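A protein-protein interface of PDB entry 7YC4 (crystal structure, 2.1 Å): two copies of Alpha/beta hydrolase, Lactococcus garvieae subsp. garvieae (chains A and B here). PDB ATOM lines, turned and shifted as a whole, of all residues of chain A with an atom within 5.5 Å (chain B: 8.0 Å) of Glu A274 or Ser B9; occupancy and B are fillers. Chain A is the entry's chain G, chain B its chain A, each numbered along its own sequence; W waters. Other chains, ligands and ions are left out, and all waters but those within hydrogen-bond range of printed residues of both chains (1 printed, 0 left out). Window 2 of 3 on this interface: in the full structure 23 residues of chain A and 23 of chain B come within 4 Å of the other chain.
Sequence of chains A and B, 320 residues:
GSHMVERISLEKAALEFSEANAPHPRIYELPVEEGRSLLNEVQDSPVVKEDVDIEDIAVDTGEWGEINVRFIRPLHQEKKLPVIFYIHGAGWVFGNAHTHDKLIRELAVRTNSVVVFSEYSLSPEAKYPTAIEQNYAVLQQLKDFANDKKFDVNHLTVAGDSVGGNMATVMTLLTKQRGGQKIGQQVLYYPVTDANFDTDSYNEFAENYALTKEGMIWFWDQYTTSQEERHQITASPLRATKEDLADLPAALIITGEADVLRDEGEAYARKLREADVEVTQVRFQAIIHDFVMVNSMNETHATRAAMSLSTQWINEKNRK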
ATOM      1  N   LYS A 242       7.382   4.994 -15.901  1.00  0.00           N
ATOM      2  CA  LYS A 242       7.759   3.564 -15.796  1.00  0.00           C
ATOM      3  C   LYS A 242       9.259   3.472 -15.452  1.00  0.00           C
ATOM      4  O   LYS A 242       9.620   2.611 -14.653  1.00  0.00           O
ATOM      5  CB  LYS A 242       7.374   2.828 -17.086  1.00  0.00           C
ATOM      6  CG  LYS A 242       7.718   1.342 -17.124  1.00  0.00           C
ATOM      7  CD  LYS A 242       8.078   0.810 -18.509  1.00  0.00           C
ATOM      8  CE  LYS A 242       8.778  -0.532 -18.471  1.00  0.00           C
ATOM      9  NZ  LYS A 242       7.914  -1.605 -19.017  1.00  0.00           N
ATOM     10  N   ALA A 269      -0.868   1.893  -7.770  1.00  0.00           N
ATOM     11  CA  ALA A 269      -0.611   0.429  -7.728  1.00  0.00           C
ATOM     12  C   ALA A 269      -0.415  -0.081  -9.164  1.00  0.00           C
ATOM     13  O   ALA A 269       0.490  -0.951  -9.392  1.00  0.00           O
ATOM     14  CB  ALA A 269      -1.724  -0.276  -7.017  1.00  0.00           C
ATOM     15  N   ARG A 270      -1.233   0.419 -10.098  1.00  0.00           N
ATOM     16  CA  ARG A 270      -1.200  -0.005 -11.529  1.00  0.00           C
ATOM     17  C   ARG A 270       0.095   0.475 -12.178  1.00  0.00           C
ATOM     18  O   ARG A 270       0.730  -0.319 -12.878  1.00  0.00           O
ATOM     19  CB  ARG A 270      -2.383   0.554 -12.322  1.00  0.00           C
ATOM     20  CG  ARG A 270      -3.724  -0.055 -11.949  1.00  0.00           C
ATOM     21  CD  ARG A 270      -4.852   0.668 -12.668  1.00  0.00           C
ATOM     22  NE  ARG A 270      -6.070  -0.128 -12.704  1.00  0.00           N
ATOM     23  CZ  ARG A 270      -7.275   0.332 -13.051  1.00  0.00           C
ATOM     24  NH1 ARG A 270      -7.434   1.595 -13.408  1.00  0.00           N
ATOM     25  NH2 ARG A 270      -8.317  -0.487 -13.053  1.00  0.00           N
ATOM     26  N   LYS A 271       0.462   1.738 -11.973  1.00  0.00           N
ATOM     27  CA  LYS A 271       1.740   2.274 -12.470  1.00  0.00           C
ATOM     28  C   LYS A 271       2.887   1.386 -11.963  1.00  0.00           C
ATOM     29  O   LYS A 271       3.681   0.997 -12.795  1.00  0.00           O
ATOM     30  CB  LYS A 271       1.871   3.752 -12.123  1.00  0.00           C
ATOM     31  CG  LYS A 271       1.111   4.658 -13.077  1.00  0.00           C
ATOM     32  CD  LYS A 271       1.991   5.692 -13.734  1.00  0.00           C
ATOM     33  CE  LYS A 271       1.279   6.992 -14.044  1.00  0.00           C
ATOM     34  NZ  LYS A 271       2.258   8.103 -14.138  1.00  0.00           N
ATOM     35  N   LEU A 272       2.964   1.044 -10.675  1.00  0.00           N
ATOM     36  CA  LEU A 272       4.060   0.169 -10.141  1.00  0.00           C
ATOM     37  C   LEU A 272       4.017  -1.203 -10.823  1.00  0.00           C
ATOM     38  O   LEU A 272       5.067  -1.698 -11.239  1.00  0.00           O
ATOM     39  CB  LEU A 272       3.916  -0.007  -8.633  1.00  0.00           C
ATOM     40  CG  LEU A 272       4.156   1.242  -7.796  1.00  0.00           C
ATOM     41  CD1 LEU A 272       3.832   0.945  -6.336  1.00  0.00           C
ATOM     42  CD2 LEU A 272       5.583   1.716  -7.963  1.00  0.00           C
ATOM     43  N   ARG A 273       2.827  -1.793 -10.939  1.00  0.00           N
ATOM     44  CA  ARG A 273       2.633  -3.073 -11.650  1.00  0.00           C
ATOM     45  C   ARG A 273       3.108  -2.944 -13.106  1.00  0.00           C
ATOM     46  O   ARG A 273       3.795  -3.845 -13.555  1.00  0.00           O
ATOM     47  CB  ARG A 273       1.177  -3.514 -11.584  1.00  0.00           C
ATOM     48  CG  ARG A 273       0.996  -4.949 -12.060  1.00  0.00           C
ATOM     49  CD  ARG A 273      -0.445  -5.429 -12.000  1.00  0.00           C
ATOM     50  NE  ARG A 273      -0.974  -5.276 -10.652  1.00  0.00           N
ATOM     51  CZ  ARG A 273      -1.802  -4.314 -10.238  1.00  0.00           C
ATOM     52  NH1 ARG A 273      -2.267  -3.411 -11.084  1.00  0.00           N
ATOM     53  NH2 ARG A 273      -2.160  -4.276  -8.964  1.00  0.00           N
ATOM     54  N   GLU A 274       2.814  -1.841 -13.790  1.00  0.00           N
ATOM     55  CA  GLU A 274       3.196  -1.649 -15.214  1.00  0.00           C
ATOM     56  C   GLU A 274       4.710  -1.441 -15.328  1.00  0.00           C
ATOM     57  O   GLU A 274       5.220  -1.701 -16.433  1.00  0.00           O
ATOM     58  CB  GLU A 274       2.383  -0.524 -15.870  1.00  0.00           C
ATOM     59  CG  GLU A 274       0.874  -0.809 -15.892  1.00  0.00           C
ATOM     60  CD  GLU A 274       0.408  -2.191 -16.357  1.00  0.00           C
ATOM     61  OE1 GLU A 274       0.681  -2.533 -17.531  1.00  0.00           O
ATOM     62  OE2 GLU A 274      -0.249  -2.924 -15.553  1.00  0.00           O
ATOM     63  N   ALA A 275       5.399  -1.023 -14.251  1.00  0.00           N
ATOM     64  CA  ALA A 275       6.877  -0.870 -14.208  1.00  0.00           C
ATOM     65  C   ALA A 275       7.554  -2.140 -13.669  1.00  0.00           C
ATOM     66  O   ALA A 275       8.752  -2.069 -13.399  1.00  0.00           O
ATOM     67  CB  ALA A 275       7.252   0.336 -13.390  1.00  0.00           C
ATOM     68  N   ASP A 276       6.812  -3.247 -13.556  1.00  0.00           N
ATOM     69  CA  ASP A 276       7.257  -4.597 -13.120  1.00  0.00           C
ATOM     70  C   ASP A 276       7.618  -4.590 -11.630  1.00  0.00           C
ATOM     71  O   ASP A 276       8.262  -5.528 -11.191  1.00  0.00           O
ATOM     72  CB  ASP A 276       8.383  -5.170 -13.989  1.00  0.00           C
ATOM     73  CG  ASP A 276       7.973  -5.456 -15.432  1.00  0.00           C
ATOM     74  OD1 ASP A 276       6.873  -6.039 -15.656  1.00  0.00           O
ATOM     75  OD2 ASP A 276       8.755  -5.098 -16.328  1.00  0.00           O
ATOM     76  N   GLU B   6      -7.383  -4.483 -25.657  1.00  0.00           N
ATOM     77  CA  GLU B   6      -7.299  -3.432 -24.614  1.00  0.00           C
ATOM     78  C   GLU B   6      -7.976  -3.970 -23.347  1.00  0.00           C
ATOM     79  O   GLU B   6      -9.136  -4.374 -23.391  1.00  0.00           O
ATOM     80  CB  GLU B   6      -7.817  -2.092 -25.140  1.00  0.00           C
ATOM     81  CG  GLU B   6      -7.210  -0.896 -24.418  1.00  0.00           C
ATOM     82  CD  GLU B   6      -6.454   0.103 -25.286  1.00  0.00           C
ATOM     83  OE1 GLU B   6      -7.121   0.900 -26.002  1.00  0.00           O
ATOM     84  OE2 GLU B   6      -5.192   0.098 -25.231  1.00  0.00           O
ATOM     85  N   ARG B   7      -7.219  -4.011 -22.259  1.00  0.00           N
ATOM     86  CA  ARG B   7      -7.612  -4.590 -20.954  1.00  0.00           C
ATOM     87  C   ARG B   7      -7.124  -3.660 -19.848  1.00  0.00           C
ATOM     88  O   ARG B   7      -6.094  -3.016 -20.054  1.00  0.00           O
ATOM     89  CB  ARG B   7      -6.919  -5.935 -20.729  1.00  0.00           C
ATOM     90  CG  ARG B   7      -7.322  -7.026 -21.710  1.00  0.00           C
ATOM     91  CD  ARG B   7      -6.781  -8.359 -21.264  1.00  0.00           C
ATOM     92  NE  ARG B   7      -7.397  -9.485 -21.947  1.00  0.00           N
ATOM     93  CZ  ARG B   7      -6.954  -9.998 -23.092  1.00  0.00           C
ATOM     94  NH1 ARG B   7      -7.547 -11.059 -23.623  1.00  0.00           N
ATOM     95  NH2 ARG B   7      -5.920  -9.448 -23.702  1.00  0.00           N
ATOM     96  N   ILE B   8      -7.789  -3.656 -18.695  1.00  0.00           N
ATOM     97  CA  ILE B   8      -7.222  -2.987 -17.491  1.00  0.00           C
ATOM     98  C   ILE B   8      -5.951  -3.740 -17.061  1.00  0.00           C
ATOM     99  O   ILE B   8      -5.712  -4.879 -17.517  1.00  0.00           O
ATOM    100  CB  ILE B   8      -8.277  -2.861 -16.380  1.00  0.00           C
ATOM    101  CG1 ILE B   8      -8.556  -4.187 -15.672  1.00  0.00           C
ATOM    102  CG2 ILE B   8      -9.550  -2.246 -16.953  1.00  0.00           C
ATOM    103  CD1 ILE B   8      -9.442  -4.030 -14.464  1.00  0.00           C
ATOM    104  N   SER B   9      -5.126  -3.078 -16.253  1.00  0.00           N
ATOM    105  CA  SER B   9      -3.904  -3.647 -15.640  1.00  0.00           C
ATOM    106  C   SER B   9      -4.247  -4.994 -14.990  1.00  0.00           C
ATOM    107  O   SER B   9      -5.172  -5.021 -14.136  1.00  0.00           O
ATOM    108  CB  SER B   9      -3.315  -2.660 -14.664  1.00  0.00           C
ATOM    109  OG  SER B   9      -2.335  -3.279 -13.841  1.00  0.00           O
ATOM    110  N   LEU B  10      -3.598  -6.084 -15.420  1.00  0.00           N
ATOM    111  CA  LEU B  10      -3.786  -7.442 -14.822  1.00  0.00           C
ATOM    112  C   LEU B  10      -2.436  -7.972 -14.333  1.00  0.00           C
ATOM    113  O   LEU B  10      -1.419  -7.571 -14.888  1.00  0.00           O
ATOM    114  CB  LEU B  10      -4.383  -8.408 -15.848  1.00  0.00           C
ATOM    115  CG  LEU B  10      -5.847  -8.168 -16.201  1.00  0.00           C
ATOM    116  CD1 LEU B  10      -6.267  -9.136 -17.285  1.00  0.00           C
ATOM    117  CD2 LEU B  10      -6.729  -8.299 -14.958  1.00  0.00           C
ATOM    118  N   GLU B  11      -2.427  -8.843 -13.329  1.00  0.00           N
ATOM    119  CA  GLU B  11      -1.214  -9.644 -13.054  1.00  0.00           C
ATOM    120  C   GLU B  11      -0.930 -10.503 -14.301  1.00  0.00           C
ATOM    121  O   GLU B  11      -1.897 -10.938 -14.968  1.00  0.00           O
ATOM    122  CB  GLU B  11      -1.365 -10.466 -11.779  1.00  0.00           C
ATOM    123  CG  GLU B  11      -1.567  -9.621 -10.541  1.00  0.00           C
ATOM    124  CD  GLU B  11      -1.206 -10.356  -9.267  1.00  0.00           C
ATOM    125  OE1 GLU B  11      -0.095 -10.933  -9.212  1.00  0.00           O
ATOM    126  OE2 GLU B  11      -2.045 -10.392  -8.364  1.00  0.00           O
ATOM    127  N   LYS B  12       0.349 -10.706 -14.615  1.00  0.00           N
ATOM    128  CA  LYS B  12       0.836 -11.434 -15.829  1.00  0.00           C
ATOM    129  C   LYS B  12       0.043 -12.739 -16.023  1.00  0.00           C
ATOM    130  O   LYS B  12      -0.517 -12.942 -17.101  1.00  0.00           O
ATOM    131  CB  LYS B  12       2.339 -11.670 -15.684  1.00  0.00           C
ATOM    132  CG  LYS B  12       3.031 -12.184 -16.940  1.00  0.00           C
ATOM    133  CD  LYS B  12       4.519 -12.434 -16.744  1.00  0.00           C
ATOM    134  CE  LYS B  12       5.184 -13.042 -17.964  1.00  0.00           C
ATOM    135  NZ  LYS B  12       6.249 -14.004 -17.590  1.00  0.00           N
ATOM    136  N   ALA B  14      -2.881 -13.672 -14.879  1.00  0.00           N
ATOM    137  CA  ALA B  14      -4.302 -13.370 -15.171  1.00  0.00           C
ATOM    138  C   ALA B  14      -4.474 -12.958 -16.650  1.00  0.00           C
ATOM    139  O   ALA B  14      -5.473 -13.407 -17.281  1.00  0.00           O
ATOM    140  CB  ALA B  14      -4.807 -12.305 -14.227  1.00  0.00           C
ATOM    141  N   LEU B  15      -3.576 -12.129 -17.184  1.00  0.00           N
ATOM    142  CA  LEU B  15      -3.536 -11.712 -18.617  1.00  0.00           C
ATOM    143  C   LEU B  15      -3.332 -12.961 -19.490  1.00  0.00           C
ATOM    144  O   LEU B  15      -4.085 -13.130 -20.486  1.00  0.00           O
ATOM    145  CB  LEU B  15      -2.427 -10.673 -18.835  1.00  0.00           C
ATOM    146  CG  LEU B  15      -2.167 -10.261 -20.293  1.00  0.00           C
ATOM    147  CD1 LEU B  15      -3.393  -9.607 -20.921  1.00  0.00           C
ATOM    148  CD2 LEU B  15      -0.957  -9.348 -20.422  1.00  0.00           C
ATOM    149  N   PHE B 205     -16.550  -6.281 -17.956  1.00  0.00           N
ATOM    150  CA  PHE B 205     -15.658  -7.471 -18.089  1.00  0.00           C
ATOM    151  C   PHE B 205     -16.389  -8.593 -18.858  1.00  0.00           C
ATOM    152  O   PHE B 205     -15.990  -9.774 -18.717  1.00  0.00           O
ATOM    153  CB  PHE B 205     -15.145  -7.889 -16.700  1.00  0.00           C
ATOM    154  CG  PHE B 205     -14.446  -6.778 -15.948  1.00  0.00           C
ATOM    155  CD1 PHE B 205     -13.196  -6.332 -16.331  1.00  0.00           C
ATOM    156  CD2 PHE B 205     -15.098  -6.098 -14.923  1.00  0.00           C
ATOM    157  CE1 PHE B 205     -12.596  -5.266 -15.671  1.00  0.00           C
ATOM    158  CE2 PHE B 205     -14.492  -5.051 -14.252  1.00  0.00           C
ATOM    159  CZ  PHE B 205     -13.240  -4.635 -14.626  1.00  0.00           C
ATOM    160  N   TYR B 209     -11.622 -11.507 -20.262  1.00  0.00           N
ATOM    161  CA  TYR B 209     -11.120 -11.765 -18.889  1.00  0.00           C
ATOM    162  C   TYR B 209     -11.416 -13.214 -18.499  1.00  0.00           C
ATOM    163  O   TYR B 209     -11.721 -13.503 -17.330  1.00  0.00           O
ATOM    164  CB  TYR B 209     -11.670 -10.699 -17.941  1.00  0.00           C
ATOM    165  CG  TYR B 209     -11.229  -9.299 -18.279  1.00  0.00           C
ATOM    166  CD1 TYR B 209     -10.066  -8.761 -17.768  1.00  0.00           C
ATOM    167  CD2 TYR B 209     -11.982  -8.516 -19.136  1.00  0.00           C
ATOM    168  CE1 TYR B 209      -9.666  -7.471 -18.089  1.00  0.00           C
ATOM    169  CE2 TYR B 209     -11.620  -7.213 -19.440  1.00  0.00           C
ATOM    170  CZ  TYR B 209     -10.466  -6.681 -18.898  1.00  0.00           C
ATOM    171  OH  TYR B 209     -10.111  -5.411 -19.228  1.00  0.00           O
ATOM    172  N   GLU B 257     -11.117  -7.665  -9.119  1.00  0.00           N
ATOM    173  CA  GLU B 257     -11.501  -6.420  -9.839  1.00  0.00           C
ATOM    174  C   GLU B 257     -12.085  -6.746 -11.223  1.00  0.00           C
ATOM    175  O   GLU B 257     -13.155  -6.156 -11.547  1.00  0.00           O
ATOM    176  CB  GLU B 257     -10.278  -5.531  -9.983  1.00  0.00           C
ATOM    177  CG  GLU B 257     -10.479  -4.322 -10.865  1.00  0.00           C
ATOM    178  CD  GLU B 257      -9.196  -3.561 -11.130  1.00  0.00           C
ATOM    179  OE1 GLU B 257      -8.113  -4.177 -11.062  1.00  0.00           O
ATOM    180  OE2 GLU B 257      -9.286  -2.362 -11.466  1.00  0.00           O
ATOM    181  N   ALA B 258     -11.416  -7.613 -12.000  1.00  0.00           N
ATOM    182  CA  ALA B 258     -11.713  -7.863 -13.427  1.00  0.00           C
ATOM    183  C   ALA B 258     -12.533  -9.151 -13.536  1.00  0.00           C
ATOM    184  O   ALA B 258     -12.039 -10.130 -14.114  1.00  0.00           O
ATOM    185  CB  ALA B 258     -10.442  -7.924 -14.223  1.00  0.00           C
ATOM    186  N   GLN B 285      -7.058  -6.201  -6.575  1.00  0.00           N
ATOM    187  CA  GLN B 285      -6.822  -5.493  -7.851  1.00  0.00           C
ATOM    188  C   GLN B 285      -6.264  -6.475  -8.899  1.00  0.00           C
ATOM    189  O   GLN B 285      -5.597  -7.463  -8.551  1.00  0.00           O
ATOM    190  CB  GLN B 285      -5.889  -4.303  -7.653  1.00  0.00           C
ATOM    191  CG  GLN B 285      -5.982  -3.276  -8.778  1.00  0.00           C
ATOM    192  CD  GLN B 285      -4.998  -2.146  -8.627  1.00  0.00           C
ATOM    193  OE1 GLN B 285      -3.796  -2.345  -8.547  1.00  0.00           O
ATOM    194  NE2 GLN B 285      -5.508  -0.929  -8.578  1.00  0.00           N
ATOM    195  N   ALA B 286      -6.557  -6.185 -10.157  1.00  0.00           N
ATOM    196  CA  ALA B 286      -5.775  -6.651 -11.320  1.00  0.00           C
ATOM    197  C   ALA B 286      -5.777  -8.183 -11.375  1.00  0.00           C
ATOM    198  O   ALA B 286      -4.791  -8.779 -11.844  1.00  0.00           O
ATOM    199  CB  ALA B 286      -4.385  -6.071 -11.243  1.00  0.00           C
ATOM    200  N   ILE B 287      -6.885  -8.799 -10.983  1.00  0.00           N
ATOM    201  CA  ILE B 287      -7.020 -10.278 -11.009  1.00  0.00           C
ATOM    202  C   ILE B 287      -8.390 -10.636 -11.572  1.00  0.00           C
ATOM    203  O   ILE B 287      -9.327  -9.808 -11.501  1.00  0.00           O
ATOM    204  CB  ILE B 287      -6.794 -10.885  -9.616  1.00  0.00           C
ATOM    205  CG1 ILE B 287      -6.373 -12.347  -9.700  1.00  0.00           C
ATOM    206  CG2 ILE B 287      -8.025 -10.702  -8.743  1.00  0.00           C
ATOM    207  CD1 ILE B 287      -5.046 -12.568 -10.354  1.00  0.00           C
ATOM    208  N   ILE B 288      -8.482 -11.833 -12.129  1.00  0.00           N
ATOM    209  CA  ILE B 288      -9.722 -12.267 -12.825  1.00  0.00           C
ATOM    210  C   ILE B 288     -10.427 -13.272 -11.930  1.00  0.00           C
ATOM    211  O   ILE B 288      -9.902 -13.614 -10.842  1.00  0.00           O
ATOM    212  CB  ILE B 288      -9.412 -12.850 -14.223  1.00  0.00           C
ATOM    213  CG1 ILE B 288      -8.402 -13.988 -14.163  1.00  0.00           C
ATOM    214  CG2 ILE B 288      -8.953 -11.757 -15.178  1.00  0.00           C
ATOM    215  CD1 ILE B 288      -8.370 -14.837 -15.413  1.00  0.00           C
HETATM  216  O   HOH W   1      -6.066  -3.036 -12.351  1.00  0.00           O
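No position is printed for both chains. Of the 10 pairs that touch across the chains among the printed residues, none has its exchanged pair printed and touching as well.
The side-chain hydroxyl of Ser B9 lies within hydrogen-bond range of the guanidinium group of Arg A273 (2.8 Å). OG of Ser B9 lies within hydrogen-bond range of OE2 of Glu A274 (2.7 Å). The side-chain carboxylate of Glu B257 is in salt-bridge range of the guanidinium group of Arg A270, at 2.6 Å. The guanidinium group of Arg A273 sits at hydrogen-bond distance from the side-chain amide oxygen of Gln B285 (2.6 Å).
The backbone NH (N) of Ile B8 lies within hydrogen-bond range of the side-chain hydroxyl (OH) of Tyr B209, at 3.0 Å. N of Glu B11 is in hydrogen-bond range of O of Ala B286 (2.8 Å). OE1 of Glu B257 lies within hydrogen-bond range of N of Ala B286 (2.7 Å).
Of the 9 printed residues of chain A, 4 touch a printed residue of chain B. Hydrophobic or aromatic side chains of chain A that line the printed part of chain B: Ala A269.
Printed residues of chain A within 4 Å of Gln B285: Ala A269 (3.3 Å), Arg A270 (3.9 Å) and Arg A273 (2.6 Å). Of the printed residues of chain A, Glu B257 touches Arg A270 (2.6 Å). Printed residues of chain B within 4 Å of Arg A273: Ser B9 (2.8 Å), Leu B10 (3.7 Å), Gln B285 (2.6 Å) and Ala B286 (3.3 Å). The nearest residue of chain B that does not touch Glu A274 is Leu B10 (4.6 Å). The nearest printed residue of chain A that does not touch Ser B9 is Ala A269 (5.8 Å). The nearest printed residue of chain A that does not touch Ile B8 is Glu A274 (6.0 Å).
Water W1 lies within hydrogen-bond range of the side-chain carboxylate of Glu B257, the backbone carbonyl oxygen of Ser B9 and the guanidinium group of Arg A270.
Ala A269 touches Gln B285. Ile B8 touches Arg A270. CB of Ser B9 touches CG of Arg A270 (3.8 Å). CG of Arg A270 touches NE2 of Gln B285, at 3.9 Å. Leu B10 touches Arg A273 (O to CD, 3.7 Å). Arg A273 touches Ala B286.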
